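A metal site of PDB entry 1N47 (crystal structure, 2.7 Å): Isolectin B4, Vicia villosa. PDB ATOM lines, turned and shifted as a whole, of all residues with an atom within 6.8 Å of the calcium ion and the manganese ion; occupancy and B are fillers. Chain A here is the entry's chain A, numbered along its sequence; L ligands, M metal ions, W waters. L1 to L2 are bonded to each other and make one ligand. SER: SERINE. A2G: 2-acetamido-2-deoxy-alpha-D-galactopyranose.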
ATOM      1  N   ASP A  85     -14.929   6.309   0.306  1.00  0.00           N
ATOM      2  CA  ASP A  85     -15.572   5.085  -0.188  1.00  0.00           C
ATOM      3  C   ASP A  85     -16.193   5.236  -1.584  1.00  0.00           C
ATOM      4  O   ASP A  85     -16.692   4.246  -2.112  1.00  0.00           O
ATOM      5  CB  ASP A  85     -16.737   4.659   0.722  1.00  0.00           C
ATOM      6  CG  ASP A  85     -16.302   3.775   1.878  1.00  0.00           C
ATOM      7  OD1 ASP A  85     -16.268   2.522   1.721  1.00  0.00           O
ATOM      8  OD2 ASP A  85     -16.018   4.256   2.998  1.00  0.00           O
ATOM      9  N   GLY A 103     -19.361   2.246   3.445  1.00  0.00           N
ATOM     10  CA  GLY A 103     -19.598   1.636   2.155  1.00  0.00           C
ATOM     11  C   GLY A 103     -21.012   1.692   1.604  1.00  0.00           C
ATOM     12  O   GLY A 103     -21.285   1.137   0.526  1.00  0.00           O
ATOM     13  N   PHE A 104     -21.920   2.329   2.329  1.00  0.00           N
ATOM     14  CA  PHE A 104     -23.301   2.468   1.858  1.00  0.00           C
ATOM     15  C   PHE A 104     -23.508   3.821   1.171  1.00  0.00           C
ATOM     16  O   PHE A 104     -24.587   4.140   0.679  1.00  0.00           O
ATOM     17  CB  PHE A 104     -24.292   2.274   2.996  1.00  0.00           C
ATOM     18  CG  PHE A 104     -24.151   0.966   3.701  1.00  0.00           C
ATOM     19  CD1 PHE A 104     -24.751  -0.190   3.189  1.00  0.00           C
ATOM     20  CD2 PHE A 104     -23.418   0.879   4.866  1.00  0.00           C
ATOM     21  CE1 PHE A 104     -24.604  -1.427   3.857  1.00  0.00           C
ATOM     22  CE2 PHE A 104     -23.267  -0.344   5.530  1.00  0.00           C
ATOM     23  CZ  PHE A 104     -23.852  -1.493   5.033  1.00  0.00           C
ATOM     24  N   LEU A 105     -22.457   4.628   1.142  1.00  0.00           N
ATOM     25  CA  LEU A 105     -22.501   5.918   0.467  1.00  0.00           C
ATOM     26  C   LEU A 105     -23.697   6.797   0.869  1.00  0.00           C
ATOM     27  O   LEU A 105     -23.984   7.770   0.184  1.00  0.00           O
ATOM     28  CB  LEU A 105     -22.503   5.707  -1.043  1.00  0.00           C
ATOM     29  CG  LEU A 105     -21.833   4.432  -1.536  1.00  0.00           C
ATOM     30  CD1 LEU A 105     -22.476   3.971  -2.812  1.00  0.00           C
ATOM     31  CD2 LEU A 105     -20.342   4.592  -1.698  1.00  0.00           C
ATOM     32  N   GLU A 123     -22.963   4.528  -9.135  1.00  0.00           N
ATOM     33  CA  GLU A 123     -21.860   4.798  -8.235  1.00  0.00           C
ATOM     34  C   GLU A 123     -20.541   4.690  -8.935  1.00  0.00           C
ATOM     35  O   GLU A 123     -20.401   3.975  -9.898  1.00  0.00           O
ATOM     36  CB  GLU A 123     -21.835   3.779  -7.079  1.00  0.00           C
ATOM     37  CG  GLU A 123     -22.181   2.335  -7.486  1.00  0.00           C
ATOM     38  CD  GLU A 123     -21.843   1.278  -6.414  1.00  0.00           C
ATOM     39  OE1 GLU A 123     -22.648   1.051  -5.486  1.00  0.00           O
ATOM     40  OE2 GLU A 123     -20.760   0.649  -6.500  1.00  0.00           O
ATOM     41  N   ASP A 125     -17.341   3.574  -7.308  1.00  0.00           N
ATOM     42  CA  ASP A 125     -16.950   2.901  -6.064  1.00  0.00           C
ATOM     43  C   ASP A 125     -15.436   2.726  -5.891  1.00  0.00           C
ATOM     44  O   ASP A 125     -14.784   2.060  -6.716  1.00  0.00           O
ATOM     45  CB  ASP A 125     -17.647   1.536  -6.096  1.00  0.00           C
ATOM     46  CG  ASP A 125     -17.825   0.925  -4.736  1.00  0.00           C
ATOM     47  OD1 ASP A 125     -17.073   1.316  -3.818  1.00  0.00           O
ATOM     48  OD2 ASP A 125     -18.679   0.035  -4.497  1.00  0.00           O
ATOM     49  N   THR A 126     -14.848   3.299  -4.831  1.00  0.00           N
ATOM     50  CA  THR A 126     -13.390   3.241  -4.668  1.00  0.00           C
ATOM     51  C   THR A 126     -12.829   2.290  -3.605  1.00  0.00           C
ATOM     52  O   THR A 126     -11.621   2.313  -3.336  1.00  0.00           O
ATOM     53  CB  THR A 126     -12.818   4.637  -4.407  1.00  0.00           C
ATOM     54  OG1 THR A 126     -13.448   5.194  -3.254  1.00  0.00           O
ATOM     55  CG2 THR A 126     -13.174   5.608  -5.533  1.00  0.00           C
ATOM     56  N   TYR A 127     -13.675   1.440  -3.006  1.00  0.00           N
ATOM     57  CA  TYR A 127     -13.175   0.524  -1.980  1.00  0.00           C
ATOM     58  C   TYR A 127     -13.974  -0.760  -1.954  1.00  0.00           C
ATOM     59  O   TYR A 127     -15.195  -0.744  -1.832  1.00  0.00           O
ATOM     60  CB  TYR A 127     -13.194   1.191  -0.599  1.00  0.00           C
ATOM     61  CG  TYR A 127     -12.850   0.259   0.547  1.00  0.00           C
ATOM     62  CD1 TYR A 127     -13.782  -0.655   1.028  1.00  0.00           C
ATOM     63  CD2 TYR A 127     -11.585   0.282   1.132  1.00  0.00           C
ATOM     64  CE1 TYR A 127     -13.475  -1.502   2.064  1.00  0.00           C
ATOM     65  CE2 TYR A 127     -11.266  -0.569   2.163  1.00  0.00           C
ATOM     66  CZ  TYR A 127     -12.223  -1.462   2.640  1.00  0.00           C
ATOM     67  OH  TYR A 127     -11.915  -2.331   3.679  1.00  0.00           O
ATOM     68  N   SER A 128     -13.282  -1.897  -2.054  1.00  0.00           N
ATOM     69  CA  SER A 128     -13.993  -3.144  -2.135  1.00  0.00           C
ATOM     70  C   SER A 128     -14.500  -3.622  -0.800  1.00  0.00           C
ATOM     71  O   SER A 128     -13.697  -3.902   0.100  1.00  0.00           O
ATOM     72  CB  SER A 128     -13.119  -4.230  -2.764  1.00  0.00           C
ATOM     73  OG  SER A 128     -12.580  -3.806  -3.994  1.00  0.00           O
ATOM     74  N   ASN A 129     -15.818  -3.700  -0.699  1.00  0.00           N
ATOM     75  CA  ASN A 129     -16.530  -4.257   0.437  1.00  0.00           C
ATOM     76  C   ASN A 129     -16.859  -5.694   0.098  1.00  0.00           C
ATOM     77  O   ASN A 129     -16.516  -6.154  -0.980  1.00  0.00           O
ATOM     78  CB  ASN A 129     -17.855  -3.520   0.676  1.00  0.00           C
ATOM     79  CG  ASN A 129     -17.662  -2.114   1.206  1.00  0.00           C
ATOM     80  OD1 ASN A 129     -17.805  -1.132   0.474  1.00  0.00           O
ATOM     81  ND2 ASN A 129     -17.347  -2.004   2.490  1.00  0.00           N
ATOM     82  N   TRP A 131     -19.617  -7.098  -0.670  1.00  0.00           N
ATOM     83  CA  TRP A 131     -20.600  -7.256  -1.757  1.00  0.00           C
ATOM     84  C   TRP A 131     -20.037  -6.794  -3.122  1.00  0.00           C
ATOM     85  O   TRP A 131     -20.700  -6.932  -4.165  1.00  0.00           O
ATOM     86  CB  TRP A 131     -21.890  -6.491  -1.417  1.00  0.00           C
ATOM     87  CG  TRP A 131     -21.611  -5.083  -0.987  1.00  0.00           C
ATOM     88  CD1 TRP A 131     -21.260  -4.024  -1.787  1.00  0.00           C
ATOM     89  CD2 TRP A 131     -21.591  -4.576   0.353  1.00  0.00           C
ATOM     90  NE1 TRP A 131     -21.035  -2.911  -1.031  1.00  0.00           N
ATOM     91  CE2 TRP A 131     -21.242  -3.220   0.296  1.00  0.00           C
ATOM     92  CE3 TRP A 131     -21.833  -5.150   1.623  1.00  0.00           C
ATOM     93  CZ2 TRP A 131     -21.136  -2.415   1.428  1.00  0.00           C
ATOM     94  CZ3 TRP A 131     -21.730  -4.358   2.736  1.00  0.00           C
ATOM     95  CH2 TRP A 131     -21.395  -3.009   2.642  1.00  0.00           C
ATOM     96  N   ASP A 132     -18.819  -6.284  -3.109  1.00  0.00           N
ATOM     97  CA  ASP A 132     -18.190  -5.736  -4.298  1.00  0.00           C
ATOM     98  C   ASP A 132     -17.192  -6.666  -4.983  1.00  0.00           C
ATOM     99  O   ASP A 132     -16.779  -7.693  -4.426  1.00  0.00           O
ATOM    100  CB  ASP A 132     -17.444  -4.456  -3.910  1.00  0.00           C
ATOM    101  CG  ASP A 132     -18.358  -3.255  -3.765  1.00  0.00           C
ATOM    102  OD1 ASP A 132     -17.916  -2.228  -3.189  1.00  0.00           O
ATOM    103  OD2 ASP A 132     -19.540  -3.250  -4.203  1.00  0.00           O
ATOM    104  N   PRO A 133     -16.842  -6.306  -6.213  1.00  0.00           N
ATOM    105  CA  PRO A 133     -15.744  -6.958  -6.945  1.00  0.00           C
ATOM    106  C   PRO A 133     -14.446  -6.443  -6.364  1.00  0.00           C
ATOM    107  O   PRO A 133     -14.471  -5.437  -5.653  1.00  0.00           O
ATOM    108  CB  PRO A 133     -15.892  -6.413  -8.360  1.00  0.00           C
ATOM    109  CG  PRO A 133     -17.244  -5.853  -8.394  1.00  0.00           C
ATOM    110  CD  PRO A 133     -17.484  -5.267  -7.020  1.00  0.00           C
ATOM    111  N   HIS A 137     -14.684   0.409  -9.445  1.00  0.00           N
ATOM    112  CA  HIS A 137     -15.689   0.148 -10.461  1.00  0.00           C
ATOM    113  C   HIS A 137     -16.849   1.112 -10.470  1.00  0.00           C
ATOM    114  O   HIS A 137     -17.136   1.796  -9.488  1.00  0.00           O
ATOM    115  CB  HIS A 137     -16.292  -1.209 -10.193  1.00  0.00           C
ATOM    116  CG  HIS A 137     -16.904  -1.313  -8.841  1.00  0.00           C
ATOM    117  ND1 HIS A 137     -16.150  -1.467  -7.704  1.00  0.00           N
ATOM    118  CD2 HIS A 137     -18.192  -1.249  -8.429  1.00  0.00           C
ATOM    119  CE1 HIS A 137     -16.945  -1.524  -6.648  1.00  0.00           C
ATOM    120  NE2 HIS A 137     -18.193  -1.396  -7.060  1.00  0.00           N
ATOM    121  N   ILE A 138     -17.549   1.103 -11.599  1.00  0.00           N
ATOM    122  CA  ILE A 138     -18.785   1.851 -11.768  1.00  0.00           C
ATOM    123  C   ILE A 138     -19.862   0.803 -11.652  1.00  0.00           C
ATOM    124  O   ILE A 138     -19.720  -0.282 -12.210  1.00  0.00           O
ATOM    125  CB  ILE A 138     -18.844   2.475 -13.145  1.00  0.00           C
ATOM    126  CG1 ILE A 138     -17.896   3.680 -13.227  1.00  0.00           C
ATOM    127  CG2 ILE A 138     -20.279   2.830 -13.491  1.00  0.00           C
ATOM    128  CD1 ILE A 138     -17.768   4.278 -14.652  1.00  0.00           C
ATOM    129  N   GLY A 139     -20.907   1.098 -10.898  1.00  0.00           N
ATOM    130  CA  GLY A 139     -21.980   0.129 -10.711  1.00  0.00           C
ATOM    131  C   GLY A 139     -23.330   0.793 -10.777  1.00  0.00           C
ATOM    132  O   GLY A 139     -23.475   1.997 -10.523  1.00  0.00           O
ATOM    133  N   ASP A 141     -26.818   0.753  -9.124  1.00  0.00           N
ATOM    134  CA  ASP A 141     -27.590   0.312  -7.985  1.00  0.00           C
ATOM    135  C   ASP A 141     -29.080   0.522  -8.174  1.00  0.00           C
ATOM    136  O   ASP A 141     -29.505   1.637  -8.382  1.00  0.00           O
ATOM    137  CB  ASP A 141     -27.110   1.095  -6.768  1.00  0.00           C
ATOM    138  CG  ASP A 141     -25.678   0.771  -6.394  1.00  0.00           C
ATOM    139  OD1 ASP A 141     -25.057   1.549  -5.647  1.00  0.00           O
ATOM    140  OD2 ASP A 141     -25.068  -0.221  -6.804  1.00  0.00           O
ATOM    141  N   ILE A 145     -27.219  -1.755  -2.323  1.00  0.00           N
ATOM    142  CA  ILE A 145     -25.789  -1.446  -2.499  1.00  0.00           C
ATOM    143  C   ILE A 145     -25.068  -2.493  -3.370  1.00  0.00           C
ATOM    144  O   ILE A 145     -23.954  -2.274  -3.830  1.00  0.00           O
ATOM    145  CB  ILE A 145     -25.138  -1.345  -1.096  1.00  0.00           C
ATOM    146  CG1 ILE A 145     -23.751  -0.735  -1.157  1.00  0.00           C
ATOM    147  CG2 ILE A 145     -25.091  -2.702  -0.410  1.00  0.00           C
ATOM    148  CD1 ILE A 145     -23.772   0.697  -1.583  1.00  0.00           C
ATOM    149  N   GLU A 146     -25.709  -3.644  -3.583  1.00  0.00           N
ATOM    150  CA  GLU A 146     -25.153  -4.733  -4.380  1.00  0.00           C
ATOM    151  C   GLU A 146     -25.590  -4.497  -5.788  1.00  0.00           C
ATOM    152  O   GLU A 146     -26.687  -4.934  -6.179  1.00  0.00           O
ATOM    153  CB  GLU A 146     -25.736  -6.073  -3.928  1.00  0.00           C
ATOM    154  CG  GLU A 146     -24.833  -7.268  -4.113  1.00  0.00           C
ATOM    155  CD  GLU A 146     -25.363  -8.541  -3.431  1.00  0.00           C
ATOM    156  OE1 GLU A 146     -25.802  -8.484  -2.231  1.00  0.00           O
ATOM    157  OE2 GLU A 146     -25.344  -9.621  -4.082  1.00  0.00           O
ATOM    158  N   SER A 147     -24.730  -3.839  -6.565  1.00  0.00           N
ATOM    159  CA  SER A 147     -25.061  -3.414  -7.930  1.00  0.00           C
ATOM    160  C   SER A 147     -25.630  -4.500  -8.805  1.00  0.00           C
ATOM    161  O   SER A 147     -25.261  -5.641  -8.711  1.00  0.00           O
ATOM    162  CB  SER A 147     -23.871  -2.789  -8.602  1.00  0.00           C
ATOM    163  OG  SER A 147     -23.407  -1.734  -7.800  1.00  0.00           O
ATOM    164  N   THR A 150     -21.870  -4.009 -12.949  1.00  0.00           N
ATOM    165  CA  THR A 150     -20.689  -3.184 -12.771  1.00  0.00           C
ATOM    166  C   THR A 150     -19.706  -3.389 -13.931  1.00  0.00           C
ATOM    167  O   THR A 150     -19.825  -4.368 -14.677  1.00  0.00           O
ATOM    168  CB  THR A 150     -19.944  -3.561 -11.493  1.00  0.00           C
ATOM    169  OG1 THR A 150     -19.388  -4.870 -11.628  1.00  0.00           O
ATOM    170  CG2 THR A 150     -20.886  -3.709 -10.306  1.00  0.00           C
HETATM  171  N   SER L   1     -13.145  -4.565   5.664  1.00  0.00           N
HETATM  172  CA  SER L   1     -14.167  -4.196   6.646  1.00  0.00           C
HETATM  173  C   SER L   1     -15.586  -4.391   6.088  1.00  0.00           C
HETATM  174  O   SER L   1     -15.777  -4.437   4.874  1.00  0.00           O
HETATM  175  CB  SER L   1     -13.941  -2.748   7.112  1.00  0.00           C
HETATM  176  OG  SER L   1     -14.504  -1.812   6.205  1.00  0.00           O
HETATM  177  OXT SER L   1     -16.546  -4.514   6.840  1.00  0.00           O
HETATM  178  O5  A2G L   2     -14.012   0.391   6.799  1.00  0.00           O
HETATM  179  C1  A2G L   2     -15.037  -0.591   6.718  1.00  0.00           C
HETATM  180  C2  A2G L   2     -16.169  -0.131   5.796  1.00  0.00           C
HETATM  181  N2  A2G L   2     -17.153  -1.173   5.808  1.00  0.00           N
HETATM  182  C3  A2G L   2     -15.616   0.100   4.411  1.00  0.00           C
HETATM  183  O3  A2G L   2     -16.672   0.586   3.596  1.00  0.00           O
HETATM  184  C4  A2G L   2     -14.565   1.174   4.520  1.00  0.00           C
HETATM  185  O4  A2G L   2     -15.213   2.359   4.987  1.00  0.00           O
HETATM  186  C5  A2G L   2     -13.490   0.784   5.527  1.00  0.00           C
HETATM  187  C6  A2G L   2     -12.577   1.975   5.757  1.00  0.00           C
HETATM  188  O6  A2G L   2     -11.307   1.497   6.212  1.00  0.00           O
HETATM  189  C7  A2G L   2     -18.425  -0.882   5.998  1.00  0.00           C
HETATM  190  O7  A2G L   2     -18.776   0.274   6.135  1.00  0.00           O
HETATM  191  C8  A2G L   2     -19.387  -2.037   6.033  1.00  0.00           C
HETATM  192 CA    CA M   1     -17.696  -0.279  -2.092  1.00  0.00          CA
HETATM  193 MN    MN M   2     -19.944  -1.178  -5.314  1.00  0.00          MN
HETATM  194  O   HOH W   1     -21.852  -0.899  -3.822  1.00  0.00           O
HETATM  195  O   HOH W   2     -21.109  -2.337  -6.648  1.00  0.00           O
HETATM  196  O   HOH W   3     -17.106   1.931  -1.091  1.00  0.00           O
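Water W1 lies within hydrogen-bond range of O of Ile 145 (2.5 Å) and OE1 of Glu 123 (2.7 Å).
Within 4 Å of the manganese ion: Glu 123, Asp 125, Asp 132 and His 137.
The side-chain carboxylate (OD1) of Asp 141 sits close to the side-chain carboxylate (OE1) of Glu 123. The backbone NH of Glu 123 sits at hydrogen-bond distance from the backbone carbonyl oxygen of Gly 139 (2.9 Å).
ND2 of Asn 129 sits at hydrogen-bond distance from O3 of A2G L2, at 2.9 Å. A nitrogen (N) of SER L1 lies within hydrogen-bond range of the side-chain hydroxyl of Tyr 127, at 3.2 Å. The backbone NH (N) of Gly 103 is in hydrogen-bond range of an oxygen (O3) of A2G L2, 3.2 Å away. O3 of A2G L2 is in hydrogen-bond range of OD1 of Asp 85, 2.7 Å away.
Within 4 Å of the calcium ion: Asp 125, Tyr 127, Asn 129 and Asp 132. The nearest printed residue that does not touch the calcium ion is Trp 131 (4.4 Å).
The manganese ion is bound by the side-chain carboxylate (OD2) of Asp 125 (1.9 Å), water W2 (2.1 Å), the side-chain carboxylate (OE2) of Glu 123 (2.3 Å), the side-chain carboxylate (OD2) of Asp 132 (2.4 Å), water W1 (2.4 Å) and a ring nitrogen (NE2) of His 137 (2.5 Å).
The calcium ion is bound by OD1 of Asp 132 (2.2 Å), OD1 of Asp 125 (2.4 Å), water W3 (2.5 Å), O of Tyr 127 (2.6 Å), OD2 of Asp 125 (2.6 Å) and OD1 of Asn 129 (2.7 Å). The calcium ion has six donor atoms within binding distance.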
